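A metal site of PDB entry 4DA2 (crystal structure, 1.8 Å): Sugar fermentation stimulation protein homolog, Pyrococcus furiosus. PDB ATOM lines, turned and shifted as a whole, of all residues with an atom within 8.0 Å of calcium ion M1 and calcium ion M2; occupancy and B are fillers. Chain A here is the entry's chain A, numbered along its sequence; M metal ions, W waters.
O of Glu 131 sits at hydrogen-bond distance from N of Val 173 (2.8 Å). NZ of Lys 133 sits close to OE2 of Glu 131 (2.8 Å).
Of the 21 residues printed, 3 come within 4 Å of calcium ion M1. The nearest printed residue that does not touch calcium ion M1 is Lys 133 (4.2 Å).
Two residues have an atom within 4 Å of calcium ion M2: Glu 109 and Asp 118. Along chain A the residues within 4 Å of calcium ion M2 span positions 109 to 118. The nearest printed residue that does not touch calcium ion M2 is Glu 131 (4.4 Å).
Calcium ion M1 is bound by the side-chain carboxylate (OD2) of Asp 118 (2.4 Å), the backbone carbonyl oxygen (O) of Thr 132 (2.4 Å), the side-chain carboxylate (OE2) of Glu 131 (2.4 Å), water W5 (2.4 Å), water W3 (2.5 Å), water W6 (2.6 Å) and the side-chain carboxylate (OD1) of Asp 118 (2.9 Å).
Water W1 binds calcium ion M2 (2.0 Å). OD1 of Asp 118 is bound to calcium ion M2. Calcium ion M2 is bound by water W6, at 2.4 Å. Calcium ion M2 is bound by water W4 (2.5 Å). The side-chain carboxylate (OE2) of Glu 109 is bound to calcium ion M2 (2.5 Å). Water W2 binds calcium ion M2. OE1 of Glu 109 is bound to calcium ion M2, 2.7 Å away. Calcium ion M2 has seven donor atoms within binding distance.
Water W4 lies within hydrogen-bond range of the backbone carbonyl oxygen of Arg 116 (2.7 Å), the side-chain carboxylate of Glu 131 (2.8 Å), the backbone NH of Asp 118 (3.4 Å) and a ring nitrogen (NE2) of His 156 (3.5 Å).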
ATOM      1  N   THR A  81      31.000 -27.315 -12.544  1.00  0.00           N
ATOM      2  CA  THR A  81      30.235 -26.616 -13.592  1.00  0.00           C
ATOM      3  C   THR A  81      29.140 -25.711 -13.020  1.00  0.00           C
ATOM      4  O   THR A  81      28.772 -24.712 -13.655  1.00  0.00           O
ATOM      5  CB  THR A  81      29.666 -27.575 -14.663  1.00  0.00           C
ATOM      6  OG1 THR A  81      28.723 -28.465 -14.056  1.00  0.00           O
ATOM      7  CG2 THR A  81      30.797 -28.359 -15.326  1.00  0.00           C
ATOM      8  N   GLN A  84      31.065 -22.568 -12.090  1.00  0.00           N
ATOM      9  CA  GLN A  84      31.325 -21.895 -13.394  1.00  0.00           C
ATOM     10  C   GLN A  84      30.064 -21.154 -13.847  1.00  0.00           C
ATOM     11  O   GLN A  84      30.127 -19.981 -14.239  1.00  0.00           O
ATOM     12  CB  GLN A  84      31.756 -22.902 -14.457  1.00  0.00           C
ATOM     13  CG  GLN A  84      33.163 -23.449 -14.271  1.00  0.00           C
ATOM     14  CD  GLN A  84      33.494 -24.457 -15.381  1.00  0.00           C
ATOM     15  OE1 GLN A  84      32.780 -24.533 -16.380  1.00  0.00           O
ATOM     16  NE2 GLN A  84      34.567 -25.194 -15.228  1.00  0.00           N
ATOM     17  N   GLY A  85      28.921 -21.841 -13.799  1.00  0.00           N
ATOM     18  CA  GLY A  85      27.639 -21.237 -14.157  1.00  0.00           C
ATOM     19  C   GLY A  85      27.305 -20.035 -13.284  1.00  0.00           C
ATOM     20  O   GLY A  85      26.822 -19.026 -13.779  1.00  0.00           O
ATOM     21  N   ARG A 108      16.228 -20.756 -17.122  1.00  0.00           N
ATOM     22  CA  ARG A 108      17.366 -21.688 -16.962  1.00  0.00           C
ATOM     23  C   ARG A 108      16.945 -23.060 -17.485  1.00  0.00           C
ATOM     24  O   ARG A 108      15.826 -23.506 -17.255  1.00  0.00           O
ATOM     25  CB  ARG A 108      17.842 -21.773 -15.527  1.00  0.00           C
ATOM     26  CG  ARG A 108      18.530 -20.496 -15.032  1.00  0.00           C
ATOM     27  CD  ARG A 108      18.600 -20.424 -13.504  1.00  0.00           C
ATOM     28  NE  ARG A 108      18.983 -19.075 -13.089  1.00  0.00           N
ATOM     29  CZ  ARG A 108      19.390 -18.759 -11.862  1.00  0.00           C
ATOM     30  NH1 ARG A 108      19.475 -19.676 -10.914  1.00  0.00           N
ATOM     31  NH2 ARG A 108      19.715 -17.497 -11.586  1.00  0.00           N
ATOM     32  N   GLU A 109      17.849 -23.720 -18.187  1.00  0.00           N
ATOM     33  CA  GLU A 109      17.581 -25.038 -18.818  1.00  0.00           C
ATOM     34  C   GLU A 109      16.315 -25.192 -19.674  1.00  0.00           C
ATOM     35  O   GLU A 109      15.634 -26.217 -19.561  1.00  0.00           O
ATOM     36  CB  GLU A 109      17.618 -26.151 -17.757  1.00  0.00           C
ATOM     37  CG  GLU A 109      18.872 -26.170 -16.912  1.00  0.00           C
ATOM     38  CD  GLU A 109      20.098 -26.567 -17.716  1.00  0.00           C
ATOM     39  OE1 GLU A 109      20.049 -27.586 -18.427  1.00  0.00           O
ATOM     40  OE2 GLU A 109      21.123 -25.863 -17.629  1.00  0.00           O
ATOM     41  N   PRO A 110      15.995 -24.197 -20.536  1.00  0.00           N
ATOM     42  CA  PRO A 110      14.832 -24.372 -21.392  1.00  0.00           C
ATOM     43  C   PRO A 110      15.048 -25.501 -22.385  1.00  0.00           C
ATOM     44  O   PRO A 110      16.176 -25.744 -22.838  1.00  0.00           O
ATOM     45  CB  PRO A 110      14.761 -23.046 -22.153  1.00  0.00           C
ATOM     46  CG  PRO A 110      16.141 -22.525 -22.131  1.00  0.00           C
ATOM     47  CD  PRO A 110      16.653 -22.898 -20.787  1.00  0.00           C
ATOM     48  N   SER A 115      16.875 -31.477 -26.645  1.00  0.00           N
ATOM     49  CA  SER A 115      17.736 -31.308 -25.499  1.00  0.00           C
ATOM     50  C   SER A 115      17.303 -30.101 -24.633  1.00  0.00           C
ATOM     51  O   SER A 115      16.162 -29.642 -24.726  1.00  0.00           O
ATOM     52  CB  SER A 115      19.181 -31.146 -26.012  1.00  0.00           C
ATOM     53  OG  SER A 115      20.116 -31.294 -24.970  1.00  0.00           O
ATOM     54  N   ARG A 116      18.211 -29.615 -23.789  1.00  0.00           N
ATOM     55  CA  ARG A 116      18.011 -28.380 -23.036  1.00  0.00           C
ATOM     56  C   ARG A 116      19.302 -27.581 -23.130  1.00  0.00           C
ATOM     57  O   ARG A 116      20.391 -28.176 -23.024  1.00  0.00           O
ATOM     58  CB  ARG A 116      17.740 -28.664 -21.548  1.00  0.00           C
ATOM     59  CG  ARG A 116      16.379 -29.339 -21.274  1.00  0.00           C
ATOM     60  CD  ARG A 116      16.165 -29.603 -19.808  1.00  0.00           C
ATOM     61  NE  ARG A 116      14.736 -29.669 -19.493  1.00  0.00           N
ATOM     62  CZ  ARG A 116      14.042 -30.784 -19.303  1.00  0.00           C
ATOM     63  NH1 ARG A 116      14.626 -31.974 -19.378  1.00  0.00           N
ATOM     64  NH2 ARG A 116      12.745 -30.699 -19.027  1.00  0.00           N
ATOM     65  N   LEU A 117      19.194 -26.277 -23.324  1.00  0.00           N
ATOM     66  CA  LEU A 117      20.394 -25.414 -23.283  1.00  0.00           C
ATOM     67  C   LEU A 117      20.389 -24.635 -21.983  1.00  0.00           C
ATOM     68  O   LEU A 117      19.345 -24.462 -21.360  1.00  0.00           O
ATOM     69  CB  LEU A 117      20.415 -24.482 -24.479  1.00  0.00           C
ATOM     70  CG  LEU A 117      20.517 -25.147 -25.854  1.00  0.00           C
ATOM     71  CD1 LEU A 117      20.410 -24.074 -26.966  1.00  0.00           C
ATOM     72  CD2 LEU A 117      21.807 -25.945 -25.971  1.00  0.00           C
ATOM     73  N   ASP A 118      21.556 -24.120 -21.581  1.00  0.00           N
ATOM     74  CA  ASP A 118      21.690 -23.527 -20.252  1.00  0.00           C
ATOM     75  C   ASP A 118      20.774 -22.362 -19.961  1.00  0.00           C
ATOM     76  O   ASP A 118      20.131 -22.332 -18.898  1.00  0.00           O
ATOM     77  CB  ASP A 118      23.125 -23.092 -19.986  1.00  0.00           C
ATOM     78  CG  ASP A 118      24.053 -24.235 -19.840  1.00  0.00           C
ATOM     79  OD1 ASP A 118      23.611 -25.344 -19.444  1.00  0.00           O
ATOM     80  OD2 ASP A 118      25.272 -24.057 -20.095  1.00  0.00           O
ATOM     81  N   TYR A 119      20.734 -21.383 -20.884  1.00  0.00           N
ATOM     82  CA  TYR A 119      19.991 -20.122 -20.626  1.00  0.00           C
ATOM     83  C   TYR A 119      19.208 -19.609 -21.809  1.00  0.00           C
ATOM     84  O   TYR A 119      19.650 -19.687 -22.955  1.00  0.00           O
ATOM     85  CB  TYR A 119      20.954 -18.994 -20.179  1.00  0.00           C
ATOM     86  CG  TYR A 119      21.911 -19.371 -19.051  1.00  0.00           C
ATOM     87  CD1 TYR A 119      21.456 -19.494 -17.735  1.00  0.00           C
ATOM     88  CD2 TYR A 119      23.258 -19.595 -19.291  1.00  0.00           C
ATOM     89  CE1 TYR A 119      22.304 -19.838 -16.697  1.00  0.00           C
ATOM     90  CE2 TYR A 119      24.147 -19.946 -18.256  1.00  0.00           C
ATOM     91  CZ  TYR A 119      23.659 -20.059 -16.957  1.00  0.00           C
ATOM     92  OH  TYR A 119      24.512 -20.419 -15.924  1.00  0.00           O
ATOM     93  N   VAL A 130      21.807 -19.257 -24.728  1.00  0.00           N
ATOM     94  CA  VAL A 130      23.240 -19.347 -24.410  1.00  0.00           C
ATOM     95  C   VAL A 130      23.559 -20.669 -23.716  1.00  0.00           C
ATOM     96  O   VAL A 130      22.931 -21.007 -22.704  1.00  0.00           O
ATOM     97  CB  VAL A 130      23.721 -18.135 -23.541  1.00  0.00           C
ATOM     98  CG1 VAL A 130      25.217 -18.283 -23.222  1.00  0.00           C
ATOM     99  CG2 VAL A 130      23.431 -16.832 -24.246  1.00  0.00           C
ATOM    100  N   GLU A 131      24.507 -21.427 -24.289  1.00  0.00           N
ATOM    101  CA  GLU A 131      25.022 -22.648 -23.677  1.00  0.00           C
ATOM    102  C   GLU A 131      26.443 -22.371 -23.185  1.00  0.00           C
ATOM    103  O   GLU A 131      27.251 -21.767 -23.926  1.00  0.00           O
ATOM    104  CB  GLU A 131      25.002 -23.814 -24.692  1.00  0.00           C
ATOM    105  CG  GLU A 131      25.631 -25.138 -24.212  1.00  0.00           C
ATOM    106  CD  GLU A 131      24.935 -25.698 -22.978  1.00  0.00           C
ATOM    107  OE1 GLU A 131      23.731 -25.422 -22.802  1.00  0.00           O
ATOM    108  OE2 GLU A 131      25.611 -26.400 -22.170  1.00  0.00           O
ATOM    109  N   THR A 132      26.719 -22.754 -21.937  1.00  0.00           N
ATOM    110  CA  THR A 132      28.072 -22.570 -21.402  1.00  0.00           C
ATOM    111  C   THR A 132      28.740 -23.923 -21.246  1.00  0.00           C
ATOM    112  O   THR A 132      28.073 -24.902 -20.847  1.00  0.00           O
ATOM    113  CB  THR A 132      28.096 -21.744 -20.102  1.00  0.00           C
ATOM    114  OG1 THR A 132      27.367 -22.447 -19.080  1.00  0.00           O
ATOM    115  CG2 THR A 132      27.464 -20.381 -20.310  1.00  0.00           C
ATOM    116  N   LYS A 133      30.012 -24.017 -21.622  1.00  0.00           N
ATOM    117  CA  LYS A 133      30.757 -25.291 -21.443  1.00  0.00           C
ATOM    118  C   LYS A 133      32.055 -25.127 -20.655  1.00  0.00           C
ATOM    119  O   LYS A 133      32.723 -24.115 -20.776  1.00  0.00           O
ATOM    120  CB  LYS A 133      31.092 -25.898 -22.803  1.00  0.00           C
ATOM    121  CG  LYS A 133      29.836 -26.202 -23.643  1.00  0.00           C
ATOM    122  CD  LYS A 133      29.581 -27.670 -23.715  1.00  0.00           C
ATOM    123  CE  LYS A 133      28.245 -27.986 -24.380  1.00  0.00           C
ATOM    124  NZ  LYS A 133      27.288 -28.373 -23.293  1.00  0.00           N
ATOM    125  N   SER A 134      32.386 -26.130 -19.849  1.00  0.00           N
ATOM    126  CA  SER A 134      33.648 -26.134 -19.121  1.00  0.00           C
ATOM    127  C   SER A 134      34.826 -26.343 -20.078  1.00  0.00           C
ATOM    128  O   SER A 134      34.814 -27.284 -20.882  1.00  0.00           O
ATOM    129  CB  SER A 134      33.654 -27.247 -18.089  1.00  0.00           C
ATOM    130  OG  SER A 134      34.904 -27.274 -17.379  1.00  0.00           O
ATOM    131  N   ARG A 152      26.273 -35.489 -25.258  1.00  0.00           N
ATOM    132  CA  ARG A 152      25.517 -34.391 -24.691  1.00  0.00           C
ATOM    133  C   ARG A 152      25.922 -33.099 -25.404  1.00  0.00           C
ATOM    134  O   ARG A 152      25.061 -32.379 -25.893  1.00  0.00           O
ATOM    135  CB  ARG A 152      25.823 -34.316 -23.185  1.00  0.00           C
ATOM    136  CG  ARG A 152      24.982 -33.382 -22.344  1.00  0.00           C
ATOM    137  CD  ARG A 152      25.679 -33.211 -20.991  1.00  0.00           C
ATOM    138  NE  ARG A 152      24.831 -32.674 -19.928  1.00  0.00           N
ATOM    139  CZ  ARG A 152      24.618 -33.260 -18.751  1.00  0.00           C
ATOM    140  NH1 ARG A 152      25.193 -34.427 -18.462  1.00  0.00           N
ATOM    141  NH2 ARG A 152      23.847 -32.682 -17.860  1.00  0.00           N
ATOM    142  N   HIS A 156      23.968 -30.484 -27.991  1.00  0.00           N
ATOM    143  CA  HIS A 156      23.809 -29.060 -27.719  1.00  0.00           C
ATOM    144  C   HIS A 156      24.263 -28.219 -28.906  1.00  0.00           C
ATOM    145  O   HIS A 156      23.572 -27.277 -29.284  1.00  0.00           O
ATOM    146  CB  HIS A 156      24.571 -28.637 -26.475  1.00  0.00           C
ATOM    147  CG  HIS A 156      24.044 -29.214 -25.197  1.00  0.00           C
ATOM    148  ND1 HIS A 156      24.797 -29.269 -24.053  1.00  0.00           N
ATOM    149  CD2 HIS A 156      22.835 -29.754 -24.889  1.00  0.00           C
ATOM    150  CE1 HIS A 156      24.070 -29.799 -23.082  1.00  0.00           C
ATOM    151  NE2 HIS A 156      22.882 -30.119 -23.562  1.00  0.00           N
ATOM    152  N   ILE A 172      27.496 -19.946 -27.790  1.00  0.00           N
ATOM    153  CA  ILE A 172      28.204 -20.851 -26.907  1.00  0.00           C
ATOM    154  C   ILE A 172      29.352 -20.131 -26.243  1.00  0.00           C
ATOM    155  O   ILE A 172      30.106 -19.400 -26.886  1.00  0.00           O
ATOM    156  CB  ILE A 172      28.647 -22.205 -27.608  1.00  0.00           C
ATOM    157  CG1 ILE A 172      29.231 -23.201 -26.596  1.00  0.00           C
ATOM    158  CG2 ILE A 172      29.636 -21.967 -28.766  1.00  0.00           C
ATOM    159  CD1 ILE A 172      29.331 -24.610 -27.166  1.00  0.00           C
ATOM    160  N   VAL A 173      29.446 -20.310 -24.932  1.00  0.00           N
ATOM    161  CA  VAL A 173      30.487 -19.647 -24.148  1.00  0.00           C
ATOM    162  C   VAL A 173      31.321 -20.706 -23.455  1.00  0.00           C
ATOM    163  O   VAL A 173      30.782 -21.464 -22.618  1.00  0.00           O
ATOM    164  CB  VAL A 173      29.885 -18.713 -23.097  1.00  0.00           C
ATOM    165  CG1 VAL A 173      31.027 -18.045 -22.278  1.00  0.00           C
ATOM    166  CG2 VAL A 173      28.979 -17.625 -23.751  1.00  0.00           C
ATOM    167  N   ILE A 175      33.967 -21.640 -20.706  1.00  0.00           N
ATOM    168  CA  ILE A 175      34.470 -21.110 -19.444  1.00  0.00           C
ATOM    169  C   ILE A 175      35.857 -21.719 -19.195  1.00  0.00           C
ATOM    170  O   ILE A 175      35.993 -22.874 -18.740  1.00  0.00           O
ATOM    171  CB  ILE A 175      33.493 -21.426 -18.270  1.00  0.00           C
ATOM    172  CG1 ILE A 175      32.061 -20.953 -18.621  1.00  0.00           C
ATOM    173  CG2 ILE A 175      34.004 -20.774 -17.002  1.00  0.00           C
ATOM    174  CD1 ILE A 175      31.921 -19.436 -18.880  1.00  0.00           C
HETATM  175 CA    CA M   1      26.307 -26.165 -19.915  1.00  0.00          CA
HETATM  176 CA    CA M   2      22.639 -27.374 -18.974  1.00  0.00          CA
HETATM  177  O   HOH W   1      23.220 -27.569 -17.018  1.00  0.00           O
HETATM  178  O   HOH W   2      21.978 -29.804 -19.596  1.00  0.00           O
HETATM  179  O   HOH W   3      26.378 -25.243 -17.638  1.00  0.00           O
HETATM  180  O   HOH W   4      22.389 -27.407 -21.452  1.00  0.00           O
HETATM  181  O   HOH W   5      27.554 -28.111 -20.625  1.00  0.00           O
HETATM  182  O   HOH W   6      24.889 -28.248 -19.230  1.00  0.00           O
